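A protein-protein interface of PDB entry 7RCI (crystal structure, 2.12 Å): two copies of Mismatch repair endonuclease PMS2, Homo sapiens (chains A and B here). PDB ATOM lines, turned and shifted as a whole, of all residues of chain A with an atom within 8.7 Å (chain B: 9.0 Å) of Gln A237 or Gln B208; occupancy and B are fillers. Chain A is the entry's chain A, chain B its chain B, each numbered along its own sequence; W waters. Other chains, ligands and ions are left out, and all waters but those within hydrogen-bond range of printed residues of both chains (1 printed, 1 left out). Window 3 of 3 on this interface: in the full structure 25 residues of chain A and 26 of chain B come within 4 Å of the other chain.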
ATOM      1  N   LYS A 224     -33.106  -5.493   7.214  1.00  0.00           N
ATOM      2  CA  LYS A 224     -32.496  -4.883   8.391  1.00  0.00           C
ATOM      3  C   LYS A 224     -31.034  -4.546   8.136  1.00  0.00           C
ATOM      4  O   LYS A 224     -30.556  -3.474   8.524  1.00  0.00           O
ATOM      5  CB  LYS A 224     -32.630  -5.816   9.594  1.00  0.00           C
ATOM      6  CG  LYS A 224     -32.157  -5.224  10.917  1.00  0.00           C
ATOM      7  CD  LYS A 224     -32.127  -6.280  12.015  1.00  0.00           C
ATOM      8  CE  LYS A 224     -31.716  -5.687  13.354  1.00  0.00           C
ATOM      9  NZ  LYS A 224     -31.698  -6.718  14.428  1.00  0.00           N
ATOM     10  N   ILE A 227     -30.642  -1.439   6.021  1.00  0.00           N
ATOM     11  CA  ILE A 227     -30.816  -0.202   6.777  1.00  0.00           C
ATOM     12  C   ILE A 227     -29.505   0.209   7.437  1.00  0.00           C
ATOM     13  O   ILE A 227     -29.173   1.398   7.506  1.00  0.00           O
ATOM     14  CB  ILE A 227     -31.952  -0.361   7.807  1.00  0.00           C
ATOM     15  CG1 ILE A 227     -33.268  -0.694   7.102  1.00  0.00           C
ATOM     16  CG2 ILE A 227     -32.118   0.906   8.631  1.00  0.00           C
ATOM     17  CD1 ILE A 227     -34.425  -0.914   8.051  1.00  0.00           C
ATOM     18  N   GLY A 228     -28.734  -0.767   7.924  1.00  0.00           N
ATOM     19  CA  GLY A 228     -27.442  -0.473   8.520  1.00  0.00           C
ATOM     20  C   GLY A 228     -26.399   0.019   7.537  1.00  0.00           C
ATOM     21  O   GLY A 228     -25.437   0.675   7.949  1.00  0.00           O
ATOM     22  N   SER A 229     -26.552  -0.303   6.252  1.00  0.00           N
ATOM     23  CA  SER A 229     -25.634   0.209   5.240  1.00  0.00           C
ATOM     24  C   SER A 229     -26.008   1.615   4.786  1.00  0.00           C
ATOM     25  O   SER A 229     -25.123   2.400   4.423  1.00  0.00           O
ATOM     26  CB  SER A 229     -25.598  -0.730   4.037  1.00  0.00           C
ATOM     27  OG  SER A 229     -25.153  -2.021   4.406  1.00  0.00           O
ATOM     28  N   VAL A 230     -27.299   1.949   4.801  1.00  0.00           N
ATOM     29  CA  VAL A 230     -27.743   3.254   4.321  1.00  0.00           C
ATOM     30  C   VAL A 230     -27.621   4.307   5.415  1.00  0.00           C
ATOM     31  O   VAL A 230     -27.192   5.438   5.156  1.00  0.00           O
ATOM     32  CB  VAL A 230     -29.184   3.157   3.787  1.00  0.00           C
ATOM     33  CG1 VAL A 230     -29.698   4.528   3.377  1.00  0.00           C
ATOM     34  CG2 VAL A 230     -29.252   2.189   2.621  1.00  0.00           C
ATOM     35  N   PHE A 231     -27.999   3.964   6.646  1.00  0.00           N
ATOM     36  CA  PHE A 231     -28.025   4.929   7.734  1.00  0.00           C
ATOM     37  C   PHE A 231     -27.087   4.594   8.887  1.00  0.00           C
ATOM     38  O   PHE A 231     -26.883   5.450   9.755  1.00  0.00           O
ATOM     39  CB  PHE A 231     -29.459   5.088   8.270  1.00  0.00           C
ATOM     40  CG  PHE A 231     -30.459   5.493   7.217  1.00  0.00           C
ATOM     41  CD1 PHE A 231     -30.455   6.777   6.694  1.00  0.00           C
ATOM     42  CD2 PHE A 231     -31.401   4.590   6.752  1.00  0.00           C
ATOM     43  CE1 PHE A 231     -31.372   7.153   5.727  1.00  0.00           C
ATOM     44  CE2 PHE A 231     -32.322   4.961   5.785  1.00  0.00           C
ATOM     45  CZ  PHE A 231     -32.306   6.243   5.272  1.00  0.00           C
ATOM     46  N   GLY A 232     -26.523   3.393   8.934  1.00  0.00           N
ATOM     47  CA  GLY A 232     -25.564   3.055   9.962  1.00  0.00           C
ATOM     48  C   GLY A 232     -26.171   2.212  11.073  1.00  0.00           C
ATOM     49  O   GLY A 232     -27.390   2.102  11.226  1.00  0.00           O
ATOM     50  N   GLN A 233     -25.286   1.604  11.871  1.00  0.00           N
ATOM     51  CA  GLN A 233     -25.725   0.791  13.001  1.00  0.00           C
ATOM     52  C   GLN A 233     -26.410   1.618  14.077  1.00  0.00           C
ATOM     53  O   GLN A 233     -27.205   1.070  14.847  1.00  0.00           O
ATOM     54  CB  GLN A 233     -24.539   0.049  13.616  1.00  0.00           C
ATOM     55  CG  GLN A 233     -24.001  -1.091  12.778  1.00  0.00           C
ATOM     56  CD  GLN A 233     -25.016  -2.198  12.602  1.00  0.00           C
ATOM     57  OE1 GLN A 233     -25.391  -2.543  11.482  1.00  0.00           O
ATOM     58  NE2 GLN A 233     -25.472  -2.764  13.714  1.00  0.00           N
ATOM     59  N   LYS A 234     -26.111   2.916  14.155  1.00  0.00           N
ATOM     60  CA  LYS A 234     -26.767   3.766  15.141  1.00  0.00           C
ATOM     61  C   LYS A 234     -28.267   3.849  14.882  1.00  0.00           C
ATOM     62  O   LYS A 234     -29.067   3.881  15.825  1.00  0.00           O
ATOM     63  CB  LYS A 234     -26.139   5.160  15.133  1.00  0.00           C
ATOM     64  N   GLN A 235     -28.668   3.889  13.610  1.00  0.00           N
ATOM     65  CA  GLN A 235     -30.089   3.949  13.285  1.00  0.00           C
ATOM     66  C   GLN A 235     -30.818   2.670  13.688  1.00  0.00           C
ATOM     67  O   GLN A 235     -31.987   2.727  14.085  1.00  0.00           O
ATOM     68  CB  GLN A 235     -30.271   4.223  11.792  1.00  0.00           C
ATOM     69  CG  GLN A 235     -31.718   4.405  11.350  1.00  0.00           C
ATOM     70  CD  GLN A 235     -32.344   5.682  11.887  1.00  0.00           C
ATOM     71  OE1 GLN A 235     -32.268   6.736  11.257  1.00  0.00           O
ATOM     72  NE2 GLN A 235     -32.977   5.588  13.052  1.00  0.00           N
ATOM     73  N   LEU A 236     -30.149   1.517  13.605  1.00  0.00           N
ATOM     74  CA  LEU A 236     -30.774   0.237  13.926  1.00  0.00           C
ATOM     75  C   LEU A 236     -31.013   0.034  15.415  1.00  0.00           C
ATOM     76  O   LEU A 236     -31.713  -0.914  15.787  1.00  0.00           O
ATOM     77  CB  LEU A 236     -29.915  -0.913  13.403  1.00  0.00           C
ATOM     78  CG  LEU A 236     -29.882  -1.106  11.891  1.00  0.00           C
ATOM     79  CD1 LEU A 236     -28.957  -2.250  11.526  1.00  0.00           C
ATOM     80  CD2 LEU A 236     -31.287  -1.373  11.384  1.00  0.00           C
ATOM     81  N   GLN A 237     -30.455   0.888  16.270  1.00  0.00           N
ATOM     82  CA  GLN A 237     -30.563   0.669  17.708  1.00  0.00           C
ATOM     83  C   GLN A 237     -31.929   1.085  18.240  1.00  0.00           C
ATOM     84  O   GLN A 237     -32.472   0.433  19.138  1.00  0.00           O
ATOM     85  CB  GLN A 237     -29.444   1.419  18.429  1.00  0.00           C
ATOM     86  CG  GLN A 237     -28.055   1.012  17.957  1.00  0.00           C
ATOM     87  CD  GLN A 237     -26.951   1.557  18.838  1.00  0.00           C
ATOM     88  OE1 GLN A 237     -27.050   2.665  19.364  1.00  0.00           O
ATOM     89  NE2 GLN A 237     -25.883   0.783  18.995  1.00  0.00           N
ATOM     90  N   SER A 238     -32.498   2.160  17.699  1.00  0.00           N
ATOM     91  CA  SER A 238     -33.775   2.685  18.155  1.00  0.00           C
ATOM     92  C   SER A 238     -34.958   2.123  17.370  1.00  0.00           C
ATOM     93  O   SER A 238     -36.033   2.733  17.367  1.00  0.00           O
ATOM     94  CB  SER A 238     -33.773   4.212  18.075  1.00  0.00           C
ATOM     95  OG  SER A 238     -33.575   4.651  16.742  1.00  0.00           O
ATOM     96  N   LEU A 239     -34.785   0.986  16.708  1.00  0.00           N
ATOM     97  CA  LEU A 239     -35.825   0.394  15.881  1.00  0.00           C
ATOM     98  C   LEU A 239     -36.346  -0.892  16.503  1.00  0.00           C
ATOM     99  O   LEU A 239     -35.612  -1.628  17.171  1.00  0.00           O
ATOM    100  CB  LEU A 239     -35.311   0.100  14.470  1.00  0.00           C
ATOM    101  CG  LEU A 239     -34.838   1.313  13.677  1.00  0.00           C
ATOM    102  CD1 LEU A 239     -34.508   0.912  12.253  1.00  0.00           C
ATOM    103  CD2 LEU A 239     -35.898   2.399  13.705  1.00  0.00           C
ATOM    104  N   ILE A 240     -37.626  -1.158  16.266  1.00  0.00           N
ATOM    105  CA  ILE A 240     -38.244  -2.421  16.655  1.00  0.00           C
ATOM    106  C   ILE A 240     -38.884  -3.029  15.415  1.00  0.00           C
ATOM    107  O   ILE A 240     -39.364  -2.292  14.540  1.00  0.00           O
ATOM    108  CB  ILE A 240     -39.269  -2.229  17.783  1.00  0.00           C
ATOM    109  CG1 ILE A 240     -40.282  -1.145  17.414  1.00  0.00           C
ATOM    110  CG2 ILE A 240     -38.568  -1.897  19.091  1.00  0.00           C
ATOM    111  CD1 ILE A 240     -41.421  -1.026  18.397  1.00  0.00           C
ATOM    112  N   ILE A 273     -39.898   0.095  12.691  1.00  0.00           N
ATOM    113  CA  ILE A 273     -40.354   1.422  13.070  1.00  0.00           C
ATOM    114  C   ILE A 273     -39.609   1.834  14.331  1.00  0.00           C
ATOM    115  O   ILE A 273     -39.117   0.996  15.091  1.00  0.00           O
ATOM    116  CB  ILE A 273     -41.881   1.479  13.287  1.00  0.00           C
ATOM    117  CG1 ILE A 273     -42.370   2.928  13.300  1.00  0.00           C
ATOM    118  CG2 ILE A 273     -42.267   0.761  14.566  1.00  0.00           C
ATOM    119  CD1 ILE A 273     -43.868   3.056  13.374  1.00  0.00           C
ATOM    120  N   SER A 274     -39.513   3.146  14.532  1.00  0.00           N
ATOM    121  CA  SER A 274     -38.830   3.677  15.699  1.00  0.00           C
ATOM    122  C   SER A 274     -39.556   3.291  16.975  1.00  0.00           C
ATOM    123  O   SER A 274     -40.768   3.052  16.987  1.00  0.00           O
ATOM    124  CB  SER A 274     -38.733   5.202  15.632  1.00  0.00           C
ATOM    125  OG  SER A 274     -37.982   5.622  14.513  1.00  0.00           O
ATOM    126  N   GLN A 275     -38.793   3.238  18.059  1.00  0.00           N
ATOM    127  CA  GLN A 275     -39.379   3.035  19.369  1.00  0.00           C
ATOM    128  C   GLN A 275     -40.173   4.274  19.761  1.00  0.00           C
ATOM    129  O   GLN A 275     -39.839   5.399  19.385  1.00  0.00           O
ATOM    130  CB  GLN A 275     -38.287   2.754  20.399  1.00  0.00           C
ATOM    131  CG  GLN A 275     -37.747   1.344  20.338  1.00  0.00           C
ATOM    132  CD  GLN A 275     -36.437   1.186  21.081  1.00  0.00           C
ATOM    133  OE1 GLN A 275     -36.208   1.820  22.110  1.00  0.00           O
ATOM    134  NE2 GLN A 275     -35.569   0.327  20.564  1.00  0.00           N
ATOM    135  N   VAL A 280     -35.878   8.862  21.246  1.00  0.00           N
ATOM    136  CA  VAL A 280     -35.301   7.972  20.242  1.00  0.00           C
ATOM    137  C   VAL A 280     -35.859   8.217  18.852  1.00  0.00           C
ATOM    138  O   VAL A 280     -35.304   7.704  17.874  1.00  0.00           O
ATOM    139  CB  VAL A 280     -35.511   6.490  20.606  1.00  0.00           C
ATOM    140  CG1 VAL A 280     -34.870   6.174  21.937  1.00  0.00           C
ATOM    141  CG2 VAL A 280     -36.990   6.138  20.599  1.00  0.00           C
ATOM    142  N   ASP B  60     -13.890  -1.615   9.297  1.00  0.00           N
ATOM    143  CA  ASP B  60     -12.787  -1.059  10.082  1.00  0.00           C
ATOM    144  C   ASP B  60     -11.476  -1.164   9.305  1.00  0.00           C
ATOM    145  O   ASP B  60     -10.452  -1.610   9.824  1.00  0.00           O
ATOM    146  CB  ASP B  60     -12.677  -1.742  11.448  1.00  0.00           C
ATOM    147  CG  ASP B  60     -13.743  -1.275  12.418  1.00  0.00           C
ATOM    148  OD1 ASP B  60     -14.335  -0.202  12.178  1.00  0.00           O
ATOM    149  OD2 ASP B  60     -13.984  -1.978  13.421  1.00  0.00           O
ATOM    150  N   GLN B 205     -16.744   0.273   5.595  1.00  0.00           N
ATOM    151  CA  GLN B 205     -17.674   0.797   6.588  1.00  0.00           C
ATOM    152  C   GLN B 205     -16.947   0.820   7.927  1.00  0.00           C
ATOM    153  O   GLN B 205     -16.327  -0.175   8.317  1.00  0.00           O
ATOM    154  CB  GLN B 205     -18.952  -0.050   6.658  1.00  0.00           C
ATOM    155  CG  GLN B 205     -20.071   0.565   7.488  1.00  0.00           C
ATOM    156  CD  GLN B 205     -21.254  -0.368   7.646  1.00  0.00           C
ATOM    157  OE1 GLN B 205     -21.333  -1.399   6.973  1.00  0.00           O
ATOM    158  NE2 GLN B 205     -22.184  -0.014   8.533  1.00  0.00           N
ATOM    159  N   LEU B 206     -17.008   1.951   8.626  1.00  0.00           N
ATOM    160  CA  LEU B 206     -16.270   2.135   9.869  1.00  0.00           C
ATOM    161  C   LEU B 206     -17.227   2.283  11.043  1.00  0.00           C
ATOM    162  O   LEU B 206     -17.987   3.255  11.112  1.00  0.00           O
ATOM    163  CB  LEU B 206     -15.348   3.350   9.779  1.00  0.00           C
ATOM    164  CG  LEU B 206     -14.378   3.355   8.598  1.00  0.00           C
ATOM    165  CD1 LEU B 206     -13.786   4.741   8.406  1.00  0.00           C
ATOM    166  CD2 LEU B 206     -13.287   2.317   8.802  1.00  0.00           C
ATOM    167  N   GLY B 207     -17.181   1.320  11.962  1.00  0.00           N
ATOM    168  CA  GLY B 207     -17.975   1.415  13.174  1.00  0.00           C
ATOM    169  C   GLY B 207     -19.461   1.378  12.892  1.00  0.00           C
ATOM    170  O   GLY B 207     -19.950   0.591  12.075  1.00  0.00           O
ATOM    171  N   GLN B 208     -20.200   2.234  13.596  1.00  0.00           N
ATOM    172  CA  GLN B 208     -21.642   2.327  13.422  1.00  0.00           C
ATOM    173  C   GLN B 208     -22.038   3.195  12.238  1.00  0.00           C
ATOM    174  O   GLN B 208     -23.234   3.430  12.042  1.00  0.00           O
ATOM    175  CB  GLN B 208     -22.294   2.868  14.696  1.00  0.00           C
ATOM    176  CG  GLN B 208     -21.745   2.286  15.994  1.00  0.00           C
ATOM    177  CD  GLN B 208     -22.133   0.832  16.221  1.00  0.00           C
ATOM    178  OE1 GLN B 208     -21.866  -0.037  15.391  1.00  0.00           O
ATOM    179  NE2 GLN B 208     -22.763   0.563  17.358  1.00  0.00           N
ATOM    180  N   GLY B 209     -21.076   3.687  11.465  1.00  0.00           N
ATOM    181  CA  GLY B 209     -21.380   4.520  10.324  1.00  0.00           C
ATOM    182  C   GLY B 209     -21.959   3.724   9.168  1.00  0.00           C
ATOM    183  O   GLY B 209     -22.155   2.509   9.228  1.00  0.00           O
ATOM    184  N   LYS B 210     -22.225   4.438   8.082  1.00  0.00           N
ATOM    185  CA  LYS B 210     -22.801   3.854   6.882  1.00  0.00           C
ATOM    186  C   LYS B 210     -21.708   3.312   5.968  1.00  0.00           C
ATOM    187  O   LYS B 210     -20.560   3.759   6.001  1.00  0.00           O
ATOM    188  CB  LYS B 210     -23.631   4.896   6.139  1.00  0.00           C
ATOM    189  CG  LYS B 210     -22.875   6.190   5.883  1.00  0.00           C
ATOM    190  CD  LYS B 210     -23.817   7.329   5.530  1.00  0.00           C
ATOM    191  CE  LYS B 210     -24.429   7.145   4.151  1.00  0.00           C
ATOM    192  NZ  LYS B 210     -23.406   7.241   3.072  1.00  0.00           N
ATOM    193  N   ARG B 211     -22.080   2.342   5.138  1.00  0.00           N
ATOM    194  CA  ARG B 211     -21.140   1.829   4.152  1.00  0.00           C
ATOM    195  C   ARG B 211     -20.887   2.882   3.079  1.00  0.00           C
ATOM    196  O   ARG B 211     -21.828   3.464   2.534  1.00  0.00           O
ATOM    197  CB  ARG B 211     -21.682   0.543   3.530  1.00  0.00           C
ATOM    198  CG  ARG B 211     -20.789  -0.040   2.460  1.00  0.00           C
ATOM    199  CD  ARG B 211     -20.994  -1.536   2.330  1.00  0.00           C
ATOM    200  NE  ARG B 211     -20.701  -2.229   3.578  1.00  0.00           N
ATOM    201  CZ  ARG B 211     -19.479  -2.528   4.000  1.00  0.00           C
ATOM    202  NH1 ARG B 211     -18.406  -2.206   3.295  1.00  0.00           N
ATOM    203  NH2 ARG B 211     -19.331  -3.159   5.160  1.00  0.00           N
HETATM  204  O   HOH W   1     -24.369   3.787   2.544  1.00  0.00           O
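No position is printed for both chains.
Along chain A the printed residues that touch a printed residue of chain B span positions 228 to 237. Among the printed residues, 10 pairs touch across the chains. Among the printed residues, no Asp or Glu carboxylate lies within 4 Å of a Lys or Arg side-chain nitrogen of the other chain.
Water W1 lies within hydrogen-bond range of O of Ser A229 (2.5 Å) and O of Arg B211 (2.6 Å).
The side-chain amide nitrogen (NE2) of Gln A275 is in hydrogen-bond range of the backbone carbonyl oxygen (O) of Gln A237 (3.4 Å). The backbone NH of Asp B60 sits at hydrogen-bond distance from the backbone carbonyl oxygen of Gln B205, 3.0 Å away. The backbone carbonyl oxygen of Gly B209 lies within hydrogen-bond range of the side-chain amide nitrogen of Gln B205 (2.6 Å). NH2 of Arg B211 sits at hydrogen-bond distance from OE1 of Gln B205 (3.2 Å).
Printed residues of chain B within 4 Å of Gln A237: Gln B208 (3.5 Å). Of chain A, only Gly A232, Gln A233, Lys A234 and Gln A237 come within 4 Å of Gln B208. Gly A232 touches two residues of chain B. Lys A234 touches just one residue of chain B: Gln B208 (3.6 Å). No residue of chain B comes within 4 Å of Ser A238. No residue of chain A comes within 4 Å of Gly B207. Of the printed residues of chain B, Val A230 touches Lys B210. Of the printed residues of chain B, Ser A229 touches Lys B210 (3.4 Å) and Arg B211 (3.1 Å). Of the printed residues of chain A, Arg B211 touches Ser A229. Of the printed residues of chain A, Lys B210 touches Ser A229 (3.4 Å) and Val A230 (3.4 Å). The nearest residue of chain A that does not touch Gln B208 is Phe A231 (4.8 Å).
The backbone carbonyl oxygen (O) of Gly A228 is in hydrogen-bond range of the side-chain amide nitrogen (NE2) of Gln B205 (3.4 Å). The backbone carbonyl oxygen of Ser A229 is in hydrogen-bond range of the backbone NH of Arg B211, 3.1 Å away. The backbone NH of Gln A233 sits at hydrogen-bond distance from the backbone carbonyl oxygen of Gln B208, 2.8 Å away.
O of Gly A228 touches O of Gly B209, at 3.97 Å. O of Ser A229 touches CB of Lys B210, 3.4 Å away. O of Val A230 touches CE of Lys B210 (3.4 Å). Gly A232 touches Gln B208. Gly B209 touches Gly A232. Gln B208 touches Lys A234 (O to N, 3.6 Å). NE2 of Gln A237 touches NE2 of Gln B208, 3.5 Å away.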
